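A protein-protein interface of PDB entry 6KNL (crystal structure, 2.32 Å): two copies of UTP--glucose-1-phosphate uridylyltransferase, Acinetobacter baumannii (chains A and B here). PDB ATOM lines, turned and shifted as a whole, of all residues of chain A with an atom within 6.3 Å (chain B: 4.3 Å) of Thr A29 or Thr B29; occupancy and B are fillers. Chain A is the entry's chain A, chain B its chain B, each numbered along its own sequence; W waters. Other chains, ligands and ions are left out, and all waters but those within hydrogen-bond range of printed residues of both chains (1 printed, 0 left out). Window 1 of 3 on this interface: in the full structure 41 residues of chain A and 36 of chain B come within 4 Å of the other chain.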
ATOM      1  N   PHE A  16      25.868 -30.248  21.273  1.00  0.00           N
ATOM      2  CA  PHE A  16      25.968 -29.453  22.530  1.00  0.00           C
ATOM      3  C   PHE A  16      26.155 -30.382  23.731  1.00  0.00           C
ATOM      4  O   PHE A  16      25.354 -30.366  24.690  1.00  0.00           O
ATOM      5  CB  PHE A  16      24.797 -28.483  22.712  1.00  0.00           C
ATOM      6  CG  PHE A  16      25.084 -27.325  23.642  1.00  0.00           C
ATOM      7  CD1 PHE A  16      26.362 -27.084  24.134  1.00  0.00           C
ATOM      8  CD2 PHE A  16      24.076 -26.447  24.007  1.00  0.00           C
ATOM      9  CE1 PHE A  16      26.618 -26.012  24.976  1.00  0.00           C
ATOM     10  CE2 PHE A  16      24.336 -25.374  24.850  1.00  0.00           C
ATOM     11  CZ  PHE A  16      25.604 -25.158  25.335  1.00  0.00           C
ATOM     12  N   ALA A  19      26.861 -30.453  27.943  1.00  0.00           N
ATOM     13  CA  ALA A  19      25.669 -29.747  28.476  1.00  0.00           C
ATOM     14  C   ALA A  19      24.435 -30.646  28.376  1.00  0.00           C
ATOM     15  O   ALA A  19      23.650 -30.647  29.327  1.00  0.00           O
ATOM     16  CB  ALA A  19      25.442 -28.439  27.752  1.00  0.00           C
ATOM     17  N   ILE A  23      20.482 -34.147  30.308  1.00  0.00           N
ATOM     18  CA  ILE A  23      19.167 -33.446  30.137  1.00  0.00           C
ATOM     19  C   ILE A  23      19.013 -33.186  28.647  1.00  0.00           C
ATOM     20  O   ILE A  23      20.016 -33.045  27.973  1.00  0.00           O
ATOM     21  CB  ILE A  23      19.078 -32.100  30.906  1.00  0.00           C
ATOM     22  CG1 ILE A  23      19.830 -31.005  30.140  1.00  0.00           C
ATOM     23  CG2 ILE A  23      19.536 -32.236  32.355  1.00  0.00           C
ATOM     24  CD1 ILE A  23      20.114 -29.751  30.909  1.00  0.00           C
ATOM     25  N   LYS A  25      18.841 -31.304  25.071  1.00  0.00           N
ATOM     26  CA  LYS A  25      19.425 -30.048  24.519  1.00  0.00           C
ATOM     27  C   LYS A  25      18.374 -28.932  24.588  1.00  0.00           C
ATOM     28  O   LYS A  25      18.775 -27.763  24.695  1.00  0.00           O
ATOM     29  CB  LYS A  25      19.901 -30.232  23.072  1.00  0.00           C
ATOM     30  CG  LYS A  25      18.794 -30.469  22.045  1.00  0.00           C
ATOM     31  CD  LYS A  25      19.191 -31.348  20.862  1.00  0.00           C
ATOM     32  CE  LYS A  25      18.068 -31.585  19.864  1.00  0.00           C
ATOM     33  NZ  LYS A  25      17.670 -30.339  19.158  1.00  0.00           N
ATOM     34  N   MET A  27      16.242 -28.271  26.822  1.00  0.00           N
ATOM     35  CA  MET A  27      16.098 -27.743  28.201  1.00  0.00           C
ATOM     36  C   MET A  27      17.347 -26.957  28.622  1.00  0.00           C
ATOM     37  O   MET A  27      17.434 -26.568  29.803  1.00  0.00           O
ATOM     38  CB  MET A  27      15.853 -28.898  29.174  1.00  0.00           C
ATOM     39  CG  MET A  27      14.586 -29.679  28.851  1.00  0.00           C
ATOM     40  SD  MET A  27      13.111 -28.633  28.859  1.00  0.00           S
ATOM     41  CE  MET A  27      13.061 -28.200  30.594  1.00  0.00           C
ATOM     42  N   VAL A  28      18.281 -26.711  27.707  1.00  0.00           N
ATOM     43  CA  VAL A  28      19.458 -25.831  27.980  1.00  0.00           C
ATOM     44  C   VAL A  28      18.956 -24.447  28.412  1.00  0.00           C
ATOM     45  O   VAL A  28      18.151 -23.830  27.658  1.00  0.00           O
ATOM     46  CB  VAL A  28      20.396 -25.731  26.764  1.00  0.00           C
ATOM     47  CG1 VAL A  28      21.174 -27.024  26.643  1.00  0.00           C
ATOM     48  N   THR A  29      19.410 -23.979  29.575  1.00  0.00           N
ATOM     49  CA  THR A  29      19.110 -22.625  30.104  1.00  0.00           C
ATOM     50  C   THR A  29      19.575 -21.583  29.091  1.00  0.00           C
ATOM     51  O   THR A  29      20.739 -21.648  28.685  1.00  0.00           O
ATOM     52  CB  THR A  29      19.752 -22.374  31.468  1.00  0.00           C
ATOM     53  OG1 THR A  29      19.647 -23.625  32.146  1.00  0.00           O
ATOM     54  N   VAL A  30      18.664 -20.688  28.701  1.00  0.00           N
ATOM     55  CA  VAL A  30      18.947 -19.455  27.918  1.00  0.00           C
ATOM     56  C   VAL A  30      18.508 -18.257  28.771  1.00  0.00           C
ATOM     57  O   VAL A  30      17.292 -17.955  28.773  1.00  0.00           O
ATOM     58  CB  VAL A  30      18.219 -19.527  26.563  1.00  0.00           C
ATOM     59  CG1 VAL A  30      18.369 -18.252  25.747  1.00  0.00           C
ATOM     60  CG2 VAL A  30      18.660 -20.747  25.766  1.00  0.00           C
ATOM     61  N   VAL A  31      19.445 -17.620  29.483  1.00  0.00           N
ATOM     62  CA  VAL A  31      19.164 -16.552  30.494  1.00  0.00           C
ATOM     63  C   VAL A  31      18.561 -17.167  31.770  1.00  0.00           C
ATOM     64  O   VAL A  31      19.252 -17.187  32.811  1.00  0.00           O
ATOM     65  CB  VAL A  31      18.216 -15.465  29.951  1.00  0.00           C
ATOM     66  CG1 VAL A  31      18.185 -14.257  30.869  1.00  0.00           C
ATOM     67  CG2 VAL A  31      18.565 -15.037  28.539  1.00  0.00           C
ATOM     68  N   ASP A  32      17.296 -17.590  31.727  1.00  0.00           N
ATOM     69  CA  ASP A  32      16.533 -17.953  32.953  1.00  0.00           C
ATOM     70  C   ASP A  32      15.492 -19.039  32.669  1.00  0.00           C
ATOM     71  O   ASP A  32      14.736 -19.367  33.602  1.00  0.00           O
ATOM     72  CB  ASP A  32      15.843 -16.722  33.549  1.00  0.00           C
ATOM     73  CG  ASP A  32      14.857 -16.051  32.607  1.00  0.00           C
ATOM     74  OD1 ASP A  32      14.897 -16.364  31.403  1.00  0.00           O
ATOM     75  OD2 ASP A  32      14.062 -15.220  33.082  1.00  0.00           O
ATOM     76  N   ARG A  33      15.471 -19.600  31.458  1.00  0.00           N
ATOM     77  CA  ARG A  33      14.489 -20.642  31.065  1.00  0.00           C
ATOM     78  C   ARG A  33      15.035 -21.513  29.939  1.00  0.00           C
ATOM     79  O   ARG A  33      15.906 -21.097  29.179  1.00  0.00           O
ATOM     80  CB  ARG A  33      13.181 -19.994  30.598  1.00  0.00           C
ATOM     81  CG  ARG A  33      13.341 -19.038  29.430  1.00  0.00           C
ATOM     82  CD  ARG A  33      13.071 -17.610  29.852  1.00  0.00           C
ATOM     83  NE  ARG A  33      11.640 -17.405  29.962  1.00  0.00           N
ATOM     84  CZ  ARG A  33      11.002 -16.890  31.007  1.00  0.00           C
ATOM     85  NH1 ARG A  33       9.685 -16.794  30.973  1.00  0.00           N
ATOM     86  NH2 ARG A  33      11.658 -16.465  32.073  1.00  0.00           N
ATOM     87  N   PRO A  34      14.488 -22.734  29.770  1.00  0.00           N
ATOM     88  CA  PRO A  34      14.889 -23.614  28.677  1.00  0.00           C
ATOM     89  C   PRO A  34      14.622 -23.040  27.278  1.00  0.00           C
ATOM     90  O   PRO A  34      13.644 -22.333  27.089  1.00  0.00           O
ATOM     91  CB  PRO A  34      14.044 -24.873  28.909  1.00  0.00           C
ATOM     92  CG  PRO A  34      12.869 -24.369  29.674  1.00  0.00           C
ATOM     93  CD  PRO A  34      13.463 -23.346  30.617  1.00  0.00           C
ATOM     94  N   ALA A  35      15.498 -23.389  26.339  1.00  0.00           N
ATOM     95  CA  ALA A  35      15.433 -22.992  24.916  1.00  0.00           C
ATOM     96  C   ALA A  35      14.019 -23.251  24.385  1.00  0.00           C
ATOM     97  O   ALA A  35      13.476 -22.354  23.717  1.00  0.00           O
ATOM     98  CB  ALA A  35      16.463 -23.747  24.119  1.00  0.00           C
ATOM     99  N   TYR A 264      24.663 -20.697  20.795  1.00  0.00           N
ATOM    100  CA  TYR A 264      24.055 -20.676  22.150  1.00  0.00           C
ATOM    101  C   TYR A 264      24.467 -19.406  22.906  1.00  0.00           C
ATOM    102  O   TYR A 264      23.586 -18.705  23.426  1.00  0.00           O
ATOM    103  CB  TYR A 264      24.502 -21.885  22.962  1.00  0.00           C
ATOM    104  CG  TYR A 264      24.146 -21.843  24.424  1.00  0.00           C
ATOM    105  CD1 TYR A 264      22.869 -22.168  24.858  1.00  0.00           C
ATOM    106  CD2 TYR A 264      25.095 -21.533  25.382  1.00  0.00           C
ATOM    107  CE1 TYR A 264      22.537 -22.163  26.203  1.00  0.00           C
ATOM    108  CE2 TYR A 264      24.780 -21.535  26.733  1.00  0.00           C
ATOM    109  CZ  TYR A 264      23.498 -21.846  27.142  1.00  0.00           C
ATOM    110  OH  TYR A 264      23.189 -21.829  28.464  1.00  0.00           O
ATOM    111  N   VAL A 268      22.237 -16.209  24.460  1.00  0.00           N
ATOM    112  CA  VAL A 268      22.234 -15.794  25.896  1.00  0.00           C
ATOM    113  C   VAL A 268      22.475 -14.282  25.941  1.00  0.00           C
ATOM    114  O   VAL A 268      21.651 -13.574  26.544  1.00  0.00           O
ATOM    115  CB  VAL A 268      23.280 -16.564  26.725  1.00  0.00           C
ATOM    116  CG1 VAL A 268      23.339 -16.077  28.164  1.00  0.00           C
ATOM    117  CG2 VAL A 268      23.032 -18.066  26.696  1.00  0.00           C
ATOM    118  N   MET B  27      21.754 -29.003  37.420  1.00  0.00           N
ATOM    119  CA  MET B  27      22.009 -29.376  35.998  1.00  0.00           C
ATOM    120  C   MET B  27      21.888 -28.166  35.061  1.00  0.00           C
ATOM    121  O   MET B  27      22.055 -28.321  33.819  1.00  0.00           O
ATOM    122  CB  MET B  27      21.026 -30.465  35.566  1.00  0.00           C
ATOM    123  CG  MET B  27      21.300 -31.770  36.273  1.00  0.00           C
ATOM    124  SD  MET B  27      23.065 -32.171  36.144  1.00  0.00           S
ATOM    125  CE  MET B  27      23.084 -32.666  34.424  1.00  0.00           C
ATOM    126  N   VAL B  28      21.593 -27.000  35.613  1.00  0.00           N
ATOM    127  CA  VAL B  28      21.397 -25.763  34.809  1.00  0.00           C
ATOM    128  C   VAL B  28      22.714 -25.494  34.085  1.00  0.00           C
ATOM    129  O   VAL B  28      23.761 -25.668  34.710  1.00  0.00           O
ATOM    130  CB  VAL B  28      20.940 -24.618  35.730  1.00  0.00           C
ATOM    131  CG1 VAL B  28      21.690 -23.326  35.496  1.00  0.00           C
ATOM    132  CG2 VAL B  28      19.437 -24.421  35.630  1.00  0.00           C
ATOM    133  N   THR B  29      22.675 -25.120  32.811  1.00  0.00           N
ATOM    134  CA  THR B  29      23.894 -25.111  31.963  1.00  0.00           C
ATOM    135  C   THR B  29      24.612 -23.777  32.161  1.00  0.00           C
ATOM    136  O   THR B  29      23.962 -22.735  32.045  1.00  0.00           O
ATOM    137  CB  THR B  29      23.641 -25.519  30.504  1.00  0.00           C
ATOM    138  OG1 THR B  29      24.196 -24.503  29.669  1.00  0.00           O
ATOM    139  CG2 THR B  29      22.187 -25.752  30.159  1.00  0.00           C
ATOM    140  N   VAL B  30      25.910 -23.870  32.478  1.00  0.00           N
ATOM    141  CA  VAL B  30      26.879 -22.757  32.676  1.00  0.00           C
ATOM    142  C   VAL B  30      27.933 -22.874  31.566  1.00  0.00           C
ATOM    143  O   VAL B  30      28.824 -23.730  31.668  1.00  0.00           O
ATOM    144  CB  VAL B  30      27.516 -22.812  34.080  1.00  0.00           C
ATOM    145  CG1 VAL B  30      28.435 -21.622  34.340  1.00  0.00           C
ATOM    146  CG2 VAL B  30      26.472 -22.930  35.180  1.00  0.00           C
ATOM    147  N   VAL B  31      27.787 -22.064  30.522  1.00  0.00           N
ATOM    148  CA  VAL B  31      28.666 -22.028  29.322  1.00  0.00           C
ATOM    149  C   VAL B  31      28.346 -23.228  28.433  1.00  0.00           C
ATOM    150  O   VAL B  31      27.738 -22.998  27.364  1.00  0.00           O
ATOM    151  CB  VAL B  31      30.159 -21.983  29.683  1.00  0.00           C
ATOM    152  CG1 VAL B  31      31.022 -22.086  28.434  1.00  0.00           C
ATOM    153  CG2 VAL B  31      30.498 -20.721  30.471  1.00  0.00           C
ATOM    154  N   ARG B  33      28.159 -26.801  30.143  1.00  0.00           N
ATOM    155  CA  ARG B  33      28.118 -27.965  31.073  1.00  0.00           C
ATOM    156  C   ARG B  33      27.254 -27.615  32.285  1.00  0.00           C
ATOM    157  O   ARG B  33      27.029 -26.447  32.601  1.00  0.00           O
ATOM    158  CB  ARG B  33      29.545 -28.387  31.469  1.00  0.00           C
ATOM    159  CG  ARG B  33      30.413 -27.275  32.051  1.00  0.00           C
ATOM    160  CD  ARG B  33      31.912 -27.542  31.973  1.00  0.00           C
ATOM    161  NE  ARG B  33      32.413 -27.488  30.603  1.00  0.00           N
ATOM    162  CZ  ARG B  33      33.011 -28.486  29.945  1.00  0.00           C
ATOM    163  NH1 ARG B  33      33.374 -28.305  28.687  1.00  0.00           N
ATOM    164  NH2 ARG B  33      33.236 -29.659  30.517  1.00  0.00           N
ATOM    165  N   TYR B 264      24.082 -16.266  38.396  1.00  0.00           N
ATOM    166  CA  TYR B 264      24.204 -17.232  37.274  1.00  0.00           C
ATOM    167  C   TYR B 264      24.673 -16.491  36.011  1.00  0.00           C
ATOM    168  O   TYR B 264      25.671 -16.921  35.409  1.00  0.00           O
ATOM    169  CB  TYR B 264      22.896 -17.994  37.054  1.00  0.00           C
ATOM    170  CG  TYR B 264      22.768 -18.670  35.712  1.00  0.00           C
ATOM    171  CD1 TYR B 264      22.238 -18.004  34.631  1.00  0.00           C
ATOM    172  CD2 TYR B 264      23.150 -19.986  35.539  1.00  0.00           C
ATOM    173  CE1 TYR B 264      22.093 -18.623  33.403  1.00  0.00           C
ATOM    174  CE2 TYR B 264      23.042 -20.617  34.311  1.00  0.00           C
ATOM    175  CZ  TYR B 264      22.507 -19.933  33.236  1.00  0.00           C
ATOM    176  OH  TYR B 264      22.386 -20.552  32.027  1.00  0.00           O
HETATM  177  O   HOH W   1      21.761 -19.071  29.906  1.00  0.00           O
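The side-chain hydroxyl of Thr A29 is in hydrogen-bond range of the backbone NH of Thr B29 (3.4 Å). The side-chain hydroxyl (OH) of Tyr A264 sits at hydrogen-bond distance from the side-chain hydroxyl (OG1) of Thr B29, at 3.1 Å.
The backbone carbonyl oxygen (O) of Val A28 is in hydrogen-bond range of the backbone NH (N) of Ala A35, at 3.0 Å. The backbone carbonyl oxygen of Thr A29 is in hydrogen-bond range of the side-chain hydroxyl of Tyr A264, at 2.5 Å. OH of Tyr B264 lies within hydrogen-bond range of O of Thr B29 (2.7 Å).
Among the printed residues, merely in contact across the chains: Val A31 with Tyr B264, Thr A29 with Tyr B264, Tyr A264 with Val B31, Val A28 with Thr B29, Thr A29 with Val B28, Phe A16 with Val B31, Ile A23 with Met B27, Tyr A264 with Tyr B264 and Ala A19 with Arg B33.
Printed residues of chain B within 4 Å of Thr A29: Val B28, Thr B29 and Tyr B264. Of the printed residues of chain B, Val A31 touches Tyr B264. Printed residues of chain A within 4 Å of Met B27: Ile A23 (3.8 Å). Of chain A, only Val A28, Thr A29 and Tyr A264 come within 4 Å of Thr B29. Printed residues of chain A within 4 Å of Val B31: Phe A16 (3.7 Å) and Tyr A264 (3.4 Å). The nearest printed residue of chain B that does not touch Thr A29 is Met B27 (5.5 Å). The nearest printed residue of chain A that does not touch Tyr B264 is Val A30 (5.0 Å).
Printed residues of chain B that touch a printed residue of chain A: Met B27, Val B28, Thr B29, Val B31, Arg B33 and Tyr B264. Hydrophobic or aromatic side chains of chain B within 4 Å of the printed part of chain A: Met B27, Val B28 and Tyr B264. Of the 15 printed residues of chain A, 7 touch a printed residue of chain B. Hydrophobic or aromatic side chains of chain A within 4 Å of the printed part of chain B: Phe A16, Ala A19, Ile A23, Val A28 and Tyr A264. Among the printed residues, 11 pairs touch across the chains. Among the printed residues, no Asp or Glu carboxylate lies within 4 Å of a Lys or Arg side-chain nitrogen of the other chain.
Val A28 touches Thr B29, and with the chains exchanged Thr A29 touches Val B28. Thr A29 touches Tyr B264, and with the chains exchanged Tyr A264 touches Thr B29. Val A31 touches Tyr B264, and with the chains exchanged Tyr A264 touches Val B31. Tyr B264 touches its own counterpart, Tyr A264. 7 positions are printed for both chains. Of the 11 pairs that touch across the chains among the printed residues, 8 have their exchanged pair printed and touching as well.
Water W1 lies within hydrogen-bond range of the side-chain hydroxyl of Tyr B264, the backbone NH of Val A31, the backbone carbonyl oxygen of Thr A29 and the side-chain hydroxyl of Tyr A264.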
